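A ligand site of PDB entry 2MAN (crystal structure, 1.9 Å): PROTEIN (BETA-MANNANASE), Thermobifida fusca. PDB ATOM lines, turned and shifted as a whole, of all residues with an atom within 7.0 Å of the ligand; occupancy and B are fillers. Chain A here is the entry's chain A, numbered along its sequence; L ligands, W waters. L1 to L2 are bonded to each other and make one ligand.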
ATOM      1  N   PRO A  27     -13.263   0.033  14.544  1.00  0.00           N
ATOM      2  CA  PRO A  27     -14.093  -0.739  15.451  1.00  0.00           C
ATOM      3  C   PRO A  27     -15.288  -1.424  14.791  1.00  0.00           C
ATOM      4  O   PRO A  27     -16.459  -1.225  15.123  1.00  0.00           O
ATOM      5  CB  PRO A  27     -14.516   0.319  16.468  1.00  0.00           C
ATOM      6  CG  PRO A  27     -14.741   1.518  15.560  1.00  0.00           C
ATOM      7  CD  PRO A  27     -13.506   1.505  14.672  1.00  0.00           C
ATOM      8  N   ASN A  29     -16.627  -4.454  14.962  1.00  0.00           N
ATOM      9  CA  ASN A  29     -17.549  -5.201  15.788  1.00  0.00           C
ATOM     10  C   ASN A  29     -18.644  -4.312  16.373  1.00  0.00           C
ATOM     11  O   ASN A  29     -19.809  -4.723  16.478  1.00  0.00           O
ATOM     12  CB  ASN A  29     -16.850  -5.894  16.969  1.00  0.00           C
ATOM     13  CG  ASN A  29     -17.857  -6.763  17.704  1.00  0.00           C
ATOM     14  OD1 ASN A  29     -18.309  -6.338  18.767  1.00  0.00           O
ATOM     15  ND2 ASN A  29     -18.213  -7.914  17.150  1.00  0.00           N
ATOM     16  N   TRP A  30     -18.234  -3.127  16.844  1.00  0.00           N
ATOM     17  CA  TRP A  30     -19.166  -2.243  17.529  1.00  0.00           C
ATOM     18  C   TRP A  30     -19.924  -1.366  16.590  1.00  0.00           C
ATOM     19  O   TRP A  30     -20.906  -0.723  16.982  1.00  0.00           O
ATOM     20  CB  TRP A  30     -18.429  -1.413  18.602  1.00  0.00           C
ATOM     21  CG  TRP A  30     -17.632  -2.336  19.503  1.00  0.00           C
ATOM     22  CD1 TRP A  30     -18.069  -3.478  20.074  1.00  0.00           C
ATOM     23  CD2 TRP A  30     -16.265  -2.168  19.917  1.00  0.00           C
ATOM     24  NE1 TRP A  30     -17.045  -4.067  20.814  1.00  0.00           N
ATOM     25  CE2 TRP A  30     -15.936  -3.261  20.727  1.00  0.00           C
ATOM     26  CE3 TRP A  30     -15.290  -1.208  19.635  1.00  0.00           C
ATOM     27  CZ2 TRP A  30     -14.667  -3.448  21.291  1.00  0.00           C
ATOM     28  CZ3 TRP A  30     -14.019  -1.361  20.194  1.00  0.00           C
ATOM     29  CH2 TRP A  30     -13.728  -2.470  21.000  1.00  0.00           C
ATOM     30  N   TYR A  31     -19.408  -1.235  15.333  1.00  0.00           N
ATOM     31  CA  TYR A  31     -20.061  -0.363  14.365  1.00  0.00           C
ATOM     32  C   TYR A  31     -20.163  -1.034  13.021  1.00  0.00           C
ATOM     33  O   TYR A  31     -19.568  -0.577  12.045  1.00  0.00           O
ATOM     34  CB  TYR A  31     -19.273   0.974  14.232  1.00  0.00           C
ATOM     35  CG  TYR A  31     -19.266   1.839  15.455  1.00  0.00           C
ATOM     36  CD1 TYR A  31     -20.264   2.765  15.757  1.00  0.00           C
ATOM     37  CD2 TYR A  31     -18.219   1.713  16.375  1.00  0.00           C
ATOM     38  CE1 TYR A  31     -20.222   3.528  16.921  1.00  0.00           C
ATOM     39  CE2 TYR A  31     -18.179   2.442  17.542  1.00  0.00           C
ATOM     40  CZ  TYR A  31     -19.173   3.373  17.794  1.00  0.00           C
ATOM     41  OH  TYR A  31     -19.078   4.127  18.951  1.00  0.00           O
ATOM     42  N   ARG A  58     -17.273 -11.580  25.087  1.00  0.00           N
ATOM     43  CA  ARG A  58     -17.705 -10.316  25.674  1.00  0.00           C
ATOM     44  C   ARG A  58     -18.650  -9.554  24.764  1.00  0.00           C
ATOM     45  O   ARG A  58     -19.546  -8.912  25.334  1.00  0.00           O
ATOM     46  CB  ARG A  58     -16.457  -9.505  26.042  1.00  0.00           C
ATOM     47  CG  ARG A  58     -16.658  -8.768  27.359  1.00  0.00           C
ATOM     48  CD  ARG A  58     -15.393  -8.019  27.755  1.00  0.00           C
ATOM     49  NE  ARG A  58     -15.787  -6.671  28.133  1.00  0.00           N
ATOM     50  CZ  ARG A  58     -15.011  -5.622  28.269  1.00  0.00           C
ATOM     51  NH1 ARG A  58     -13.712  -5.711  28.051  1.00  0.00           N
ATOM     52  NH2 ARG A  58     -15.575  -4.462  28.606  1.00  0.00           N
ATOM     53  N   TRP A  59     -18.494  -9.571  23.455  1.00  0.00           N
ATOM     54  CA  TRP A  59     -19.402  -8.809  22.566  1.00  0.00           C
ATOM     55  C   TRP A  59     -20.093  -9.824  21.671  1.00  0.00           C
ATOM     56  O   TRP A  59     -20.015 -11.031  21.998  1.00  0.00           O
ATOM     57  CB  TRP A  59     -18.622  -7.752  21.783  1.00  0.00           C
ATOM     58  CG  TRP A  59     -18.095  -6.678  22.707  1.00  0.00           C
ATOM     59  CD1 TRP A  59     -18.862  -5.692  23.286  1.00  0.00           C
ATOM     60  CD2 TRP A  59     -16.778  -6.510  23.236  1.00  0.00           C
ATOM     61  NE1 TRP A  59     -18.111  -4.918  24.095  1.00  0.00           N
ATOM     62  CE2 TRP A  59     -16.818  -5.405  24.096  1.00  0.00           C
ATOM     63  CE3 TRP A  59     -15.578  -7.197  23.032  1.00  0.00           C
ATOM     64  CZ2 TRP A  59     -15.688  -4.936  24.775  1.00  0.00           C
ATOM     65  CZ3 TRP A  59     -14.466  -6.753  23.728  1.00  0.00           C
ATOM     66  CH2 TRP A  59     -14.526  -5.638  24.566  1.00  0.00           C
ATOM     67  N   HIS A  86     -11.010  -8.892  20.201  1.00  0.00           N
ATOM     68  CA  HIS A  86     -10.889  -7.906  21.266  1.00  0.00           C
ATOM     69  C   HIS A  86     -11.291  -8.396  22.643  1.00  0.00           C
ATOM     70  O   HIS A  86     -10.891  -7.812  23.641  1.00  0.00           O
ATOM     71  CB  HIS A  86     -11.788  -6.684  20.964  1.00  0.00           C
ATOM     72  CG  HIS A  86     -11.181  -5.410  21.502  1.00  0.00           C
ATOM     73  ND1 HIS A  86     -10.175  -4.783  20.789  1.00  0.00           N
ATOM     74  CD2 HIS A  86     -11.394  -4.677  22.627  1.00  0.00           C
ATOM     75  CE1 HIS A  86      -9.835  -3.689  21.441  1.00  0.00           C
ATOM     76  NE2 HIS A  86     -10.528  -3.629  22.549  1.00  0.00           N
ATOM     77  N   THR A  89      -9.038  -8.696  26.126  1.00  0.00           N
ATOM     78  CA  THR A  89      -8.534  -7.506  26.788  1.00  0.00           C
ATOM     79  C   THR A  89      -8.537  -7.537  28.301  1.00  0.00           C
ATOM     80  O   THR A  89      -9.624  -7.649  28.904  1.00  0.00           O
ATOM     81  CB  THR A  89      -9.287  -6.241  26.288  1.00  0.00           C
ATOM     82  OG1 THR A  89      -9.209  -6.130  24.843  1.00  0.00           O
ATOM     83  CG2 THR A  89      -8.678  -5.011  26.937  1.00  0.00           C
ATOM     84  N   GLN A  94      -9.755  -7.690  34.122  1.00  0.00           N
ATOM     85  CA  GLN A  94     -11.063  -7.343  33.568  1.00  0.00           C
ATOM     86  C   GLN A  94     -12.065  -8.485  33.715  1.00  0.00           C
ATOM     87  O   GLN A  94     -11.837  -9.600  33.211  1.00  0.00           O
ATOM     88  CB  GLN A  94     -10.885  -6.982  32.073  1.00  0.00           C
ATOM     89  CG  GLN A  94     -12.152  -6.830  31.264  1.00  0.00           C
ATOM     90  CD  GLN A  94     -12.919  -5.578  31.684  1.00  0.00           C
ATOM     91  OE1 GLN A  94     -12.341  -4.482  31.780  1.00  0.00           O
ATOM     92  NE2 GLN A  94     -14.205  -5.754  31.940  1.00  0.00           N
ATOM     93  N   ASN A 127      -6.282  -9.136  21.556  1.00  0.00           N
ATOM     94  CA  ASN A 127      -5.859  -7.807  21.974  1.00  0.00           C
ATOM     95  C   ASN A 127      -5.460  -7.807  23.453  1.00  0.00           C
ATOM     96  O   ASN A 127      -6.109  -8.421  24.298  1.00  0.00           O
ATOM     97  CB  ASN A 127      -7.073  -6.874  21.843  1.00  0.00           C
ATOM     98  CG  ASN A 127      -6.714  -5.438  22.142  1.00  0.00           C
ATOM     99  OD1 ASN A 127      -5.914  -4.843  21.406  1.00  0.00           O
ATOM    100  ND2 ASN A 127      -7.301  -4.819  23.155  1.00  0.00           N
ATOM    101  N   GLU A 128      -4.367  -7.132  23.781  1.00  0.00           N
ATOM    102  CA  GLU A 128      -3.958  -6.891  25.181  1.00  0.00           C
ATOM    103  C   GLU A 128      -4.438  -7.974  26.137  1.00  0.00           C
ATOM    104  O   GLU A 128      -5.262  -7.711  27.029  1.00  0.00           O
ATOM    105  CB  GLU A 128      -4.631  -5.562  25.605  1.00  0.00           C
ATOM    106  CG  GLU A 128      -4.196  -4.398  24.726  1.00  0.00           C
ATOM    107  CD  GLU A 128      -4.707  -3.033  25.095  1.00  0.00           C
ATOM    108  OE1 GLU A 128      -5.509  -2.875  26.049  1.00  0.00           O
ATOM    109  OE2 GLU A 128      -4.290  -2.037  24.463  1.00  0.00           O
ATOM    110  N   TRP A 167      -2.042  -4.760  29.918  1.00  0.00           N
ATOM    111  CA  TRP A 167      -2.977  -4.090  29.019  1.00  0.00           C
ATOM    112  C   TRP A 167      -2.255  -3.646  27.752  1.00  0.00           C
ATOM    113  O   TRP A 167      -2.485  -2.534  27.295  1.00  0.00           O
ATOM    114  CB  TRP A 167      -3.652  -2.864  29.662  1.00  0.00           C
ATOM    115  CG  TRP A 167      -4.423  -3.173  30.913  1.00  0.00           C
ATOM    116  CD1 TRP A 167      -3.943  -3.255  32.180  1.00  0.00           C
ATOM    117  CD2 TRP A 167      -5.829  -3.446  30.981  1.00  0.00           C
ATOM    118  NE1 TRP A 167      -4.971  -3.561  33.040  1.00  0.00           N
ATOM    119  CE2 TRP A 167      -6.138  -3.672  32.319  1.00  0.00           C
ATOM    120  CE3 TRP A 167      -6.843  -3.473  30.007  1.00  0.00           C
ATOM    121  CZ2 TRP A 167      -7.435  -3.961  32.752  1.00  0.00           C
ATOM    122  CZ3 TRP A 167      -8.138  -3.784  30.450  1.00  0.00           C
ATOM    123  CH2 TRP A 167      -8.440  -3.978  31.820  1.00  0.00           C
ATOM    124  N   TRP A 254      -4.670   4.272  17.181  1.00  0.00           N
ATOM    125  CA  TRP A 254      -6.044   3.999  17.662  1.00  0.00           C
ATOM    126  C   TRP A 254      -6.744   5.351  17.778  1.00  0.00           C
ATOM    127  O   TRP A 254      -6.168   6.215  18.420  1.00  0.00           O
ATOM    128  CB  TRP A 254      -5.960   3.340  19.077  1.00  0.00           C
ATOM    129  CG  TRP A 254      -7.331   2.972  19.584  1.00  0.00           C
ATOM    130  CD1 TRP A 254      -8.167   3.817  20.273  1.00  0.00           C
ATOM    131  CD2 TRP A 254      -8.044   1.728  19.456  1.00  0.00           C
ATOM    132  NE1 TRP A 254      -9.358   3.170  20.583  1.00  0.00           N
ATOM    133  CE2 TRP A 254      -9.299   1.890  20.078  1.00  0.00           C
ATOM    134  CE3 TRP A 254      -7.754   0.500  18.859  1.00  0.00           C
ATOM    135  CZ2 TRP A 254     -10.268   0.890  20.108  1.00  0.00           C
ATOM    136  CZ3 TRP A 254      -8.699  -0.515  18.933  1.00  0.00           C
ATOM    137  CH2 TRP A 254      -9.952  -0.320  19.537  1.00  0.00           C
ATOM    138  N   SER A 255      -7.925   5.567  17.203  1.00  0.00           N
ATOM    139  CA  SER A 255      -8.611   4.639  16.312  1.00  0.00           C
ATOM    140  C   SER A 255      -9.431   5.515  15.338  1.00  0.00           C
ATOM    141  O   SER A 255      -9.621   6.706  15.577  1.00  0.00           O
ATOM    142  CB  SER A 255      -9.577   3.632  16.934  1.00  0.00           C
ATOM    143  OG  SER A 255     -10.670   4.332  17.549  1.00  0.00           O
ATOM    144  N   SER A 257     -12.737   6.109  14.582  1.00  0.00           N
ATOM    145  CA  SER A 257     -13.829   6.898  15.165  1.00  0.00           C
ATOM    146  C   SER A 257     -14.631   6.051  16.137  1.00  0.00           C
ATOM    147  O   SER A 257     -14.330   4.871  16.346  1.00  0.00           O
ATOM    148  CB  SER A 257     -14.727   7.483  14.061  1.00  0.00           C
ATOM    149  OG  SER A 257     -15.450   8.657  14.433  1.00  0.00           O
ATOM    150  N   GLY A 258     -15.570   6.667  16.853  1.00  0.00           N
ATOM    151  CA  GLY A 258     -16.474   5.953  17.718  1.00  0.00           C
ATOM    152  C   GLY A 258     -15.960   5.541  19.074  1.00  0.00           C
ATOM    153  O   GLY A 258     -16.540   4.632  19.675  1.00  0.00           O
ATOM    154  N   ASN A 259     -14.834   6.221  19.557  1.00  0.00           N
ATOM    155  CA  ASN A 259     -14.389   5.864  20.893  1.00  0.00           C
ATOM    156  C   ASN A 259     -15.464   6.262  21.920  1.00  0.00           C
ATOM    157  O   ASN A 259     -16.028   7.344  21.789  1.00  0.00           O
ATOM    158  CB  ASN A 259     -13.103   6.631  21.251  1.00  0.00           C
ATOM    159  CG  ASN A 259     -11.937   5.836  20.654  1.00  0.00           C
ATOM    160  OD1 ASN A 259     -11.652   4.751  21.129  1.00  0.00           O
ATOM    161  ND2 ASN A 259     -11.341   6.378  19.619  1.00  0.00           N
ATOM    162  N   GLY A 260     -15.630   5.516  22.920  1.00  0.00           N
ATOM    163  CA  GLY A 260     -16.536   5.861  24.023  1.00  0.00           C
ATOM    164  C   GLY A 260     -15.634   5.782  25.281  1.00  0.00           C
ATOM    165  O   GLY A 260     -14.405   6.039  25.237  1.00  0.00           O
ATOM    166  N   GLY A 261     -16.216   5.418  26.402  1.00  0.00           N
ATOM    167  CA  GLY A 261     -15.587   5.209  27.655  1.00  0.00           C
ATOM    168  C   GLY A 261     -14.503   6.161  28.106  1.00  0.00           C
ATOM    169  O   GLY A 261     -13.491   5.704  28.667  1.00  0.00           O
ATOM    170  N   GLY A 262     -14.699   7.457  27.884  1.00  0.00           N
ATOM    171  CA  GLY A 262     -13.723   8.447  28.310  1.00  0.00           C
ATOM    172  C   GLY A 262     -12.660   8.791  27.303  1.00  0.00           C
ATOM    173  O   GLY A 262     -12.166   9.924  27.373  1.00  0.00           O
ATOM    174  N   VAL A 263     -12.305   7.886  26.318  1.00  0.00           N
ATOM    175  CA  VAL A 263     -11.252   8.198  25.371  1.00  0.00           C
ATOM    176  C   VAL A 263     -11.715   8.720  24.038  1.00  0.00           C
ATOM    177  O   VAL A 263     -11.094   8.405  23.004  1.00  0.00           O
ATOM    178  CB  VAL A 263     -10.298   6.995  25.165  1.00  0.00           C
ATOM    179  CG1 VAL A 263      -9.566   6.724  26.482  1.00  0.00           C
ATOM    180  CG2 VAL A 263     -11.073   5.789  24.678  1.00  0.00           C
ATOM    181  N   GLU A 264     -12.803   9.577  24.015  1.00  0.00           N
ATOM    182  CA  GLU A 264     -13.332  10.181  22.807  1.00  0.00           C
ATOM    183  C   GLU A 264     -12.330  11.017  22.041  1.00  0.00           C
ATOM    184  O   GLU A 264     -12.423  11.164  20.821  1.00  0.00           O
ATOM    185  CB  GLU A 264     -14.554  11.053  23.146  1.00  0.00           C
ATOM    186  N   LEU A 266      -9.427  10.070  21.190  1.00  0.00           N
ATOM    187  CA  LEU A 266      -8.688   9.165  20.288  1.00  0.00           C
ATOM    188  C   LEU A 266      -9.380   8.989  18.953  1.00  0.00           C
ATOM    189  O   LEU A 266      -8.829   8.311  18.061  1.00  0.00           O
ATOM    190  CB  LEU A 266      -8.425   7.842  21.004  1.00  0.00           C
ATOM    191  CG  LEU A 266      -7.470   7.918  22.208  1.00  0.00           C
ATOM    192  CD1 LEU A 266      -7.214   6.534  22.796  1.00  0.00           C
ATOM    193  CD2 LEU A 266      -6.118   8.521  21.802  1.00  0.00           C
HETATM  194  C1  LIG L   1     -11.585   1.905  24.731  1.00  0.00           C
HETATM  195  C2  LIG L   1     -12.625   2.652  23.845  1.00  0.00           C
HETATM  196  C3  LIG L   1     -14.003   2.080  24.154  1.00  0.00           C
HETATM  197  C4  LIG L   1     -14.027   0.587  23.924  1.00  0.00           C
HETATM  198  C5  LIG L   1     -12.874  -0.109  24.697  1.00  0.00           C
HETATM  199  C6  LIG L   1     -12.802  -1.582  24.343  1.00  0.00           C
HETATM  200  O1  LIG L   1     -12.331   2.479  22.468  1.00  0.00           O
HETATM  201  O2  LIG L   1     -14.965   2.705  23.303  1.00  0.00           O
HETATM  202  O3  LIG L   1     -15.231  -0.007  24.328  1.00  0.00           O
HETATM  203  O4  LIG L   1     -11.643   0.527  24.374  1.00  0.00           O
HETATM  204  O5  LIG L   1     -11.973  -2.231  25.269  1.00  0.00           O
HETATM  205  C1  LG2 L   2     -16.297  -0.224  23.448  1.00  0.00           C
HETATM  206  C2  LG2 L   2     -17.375  -1.123  24.094  1.00  0.00           C
HETATM  207  C3  LG2 L   2     -18.454  -1.341  23.051  1.00  0.00           C
HETATM  208  C4  LG2 L   2     -19.025  -0.026  22.572  1.00  0.00           C
HETATM  209  C5  LG2 L   2     -17.856   0.810  21.983  1.00  0.00           C
HETATM  210  C6  LG2 L   2     -18.219   2.185  21.467  1.00  0.00           C
HETATM  211  O1  LG2 L   2     -17.896  -0.480  25.246  1.00  0.00           O
HETATM  212  O2  LG2 L   2     -19.467  -2.164  23.637  1.00  0.00           O
HETATM  213  O3  LG2 L   2     -20.030  -0.256  21.615  1.00  0.00           O
HETATM  214  O4  LG2 L   2     -16.861   0.990  23.003  1.00  0.00           O
HETATM  215  O5  LG2 L   2     -18.709   2.925  22.565  1.00  0.00           O
HETATM  216  O   HOH W   1     -14.392   2.221  20.167  1.00  0.00           O
HETATM  217  O   HOH W   2     -18.211   2.186  25.333  1.00  0.00           O
HETATM  218  O   HOH W   3     -18.773  -3.133  27.207  1.00  0.00           O
HETATM  219  O   HOH W   4      -9.336  -1.326  24.393  1.00  0.00           O
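Water W4 lies within hydrogen-bond range of an oxygen (O5) of LIG L1 (2.9 Å) and a ring nitrogen (NE2) of His 86 (3.2 Å).
Water W1 bridges O1 of LIG L1 and O of Gly 258.
The side-chain amide oxygen of Asn 259 lies within hydrogen-bond range of the indole nitrogen of Trp 254 (2.8 Å).
OG of Ser 255 lies within hydrogen-bond range of ND2 of Asn 259 (3.0 Å).
The backbone carbonyl oxygen of Gly 258 sits at hydrogen-bond distance from the side-chain hydroxyl of Tyr 31 (2.7 Å).
A ring nitrogen (NE2) of His 86 sits close to the side-chain amide nitrogen (ND2) of Asn 127 (3.5 Å).
The backbone carbonyl oxygen (O) of His 86 is in hydrogen-bond range of the side-chain hydroxyl (OG1) of Thr 89.
The indole nitrogen (NE1) of Trp 30 sits close to the side-chain amide oxygen (OD1) of Asn 29 (3.3 Å).
CH2 of Trp 30 touches C6 of LIG L1, at 3.6 Å.
OH of Tyr 31 touches C6 of LG2 L2 (3.3 Å).
CZ2 of Trp 254 touches O1 of LIG L1, at 3.5 Å.
O of Gly 258 touches C6 of LG2 L2, 3.5 Å away.
CG2 of Val 263 touches C2 of LIG L1, 3.6 Å away.
Hydrophobic or aromatic side chains within 4 Å of the ligand: Trp 30, Tyr 31, Trp 59, His 86, Trp 254 and Val 263.
Of the 23 residues printed, 9 come within 4 Å of the ligand.
The nearest printed residue that does not touch the ligand is Gly 261 (4.3 Å).
A ring nitrogen (NE2) of His 86 is in hydrogen-bond range of an oxygen (O5) of LIG L1 (3.4 Å).
The side-chain amide oxygen of Asn 259 is in hydrogen-bond range of an oxygen (O1) of LIG L1 (2.7 Å).
N of Gly 260 sits at hydrogen-bond distance from O2 of LIG L1 (2.9 Å).
An oxygen (O2) of LG2 L2 lies within hydrogen-bond range of the indole nitrogen (NE1) of Trp 59, at 3.1 Å.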
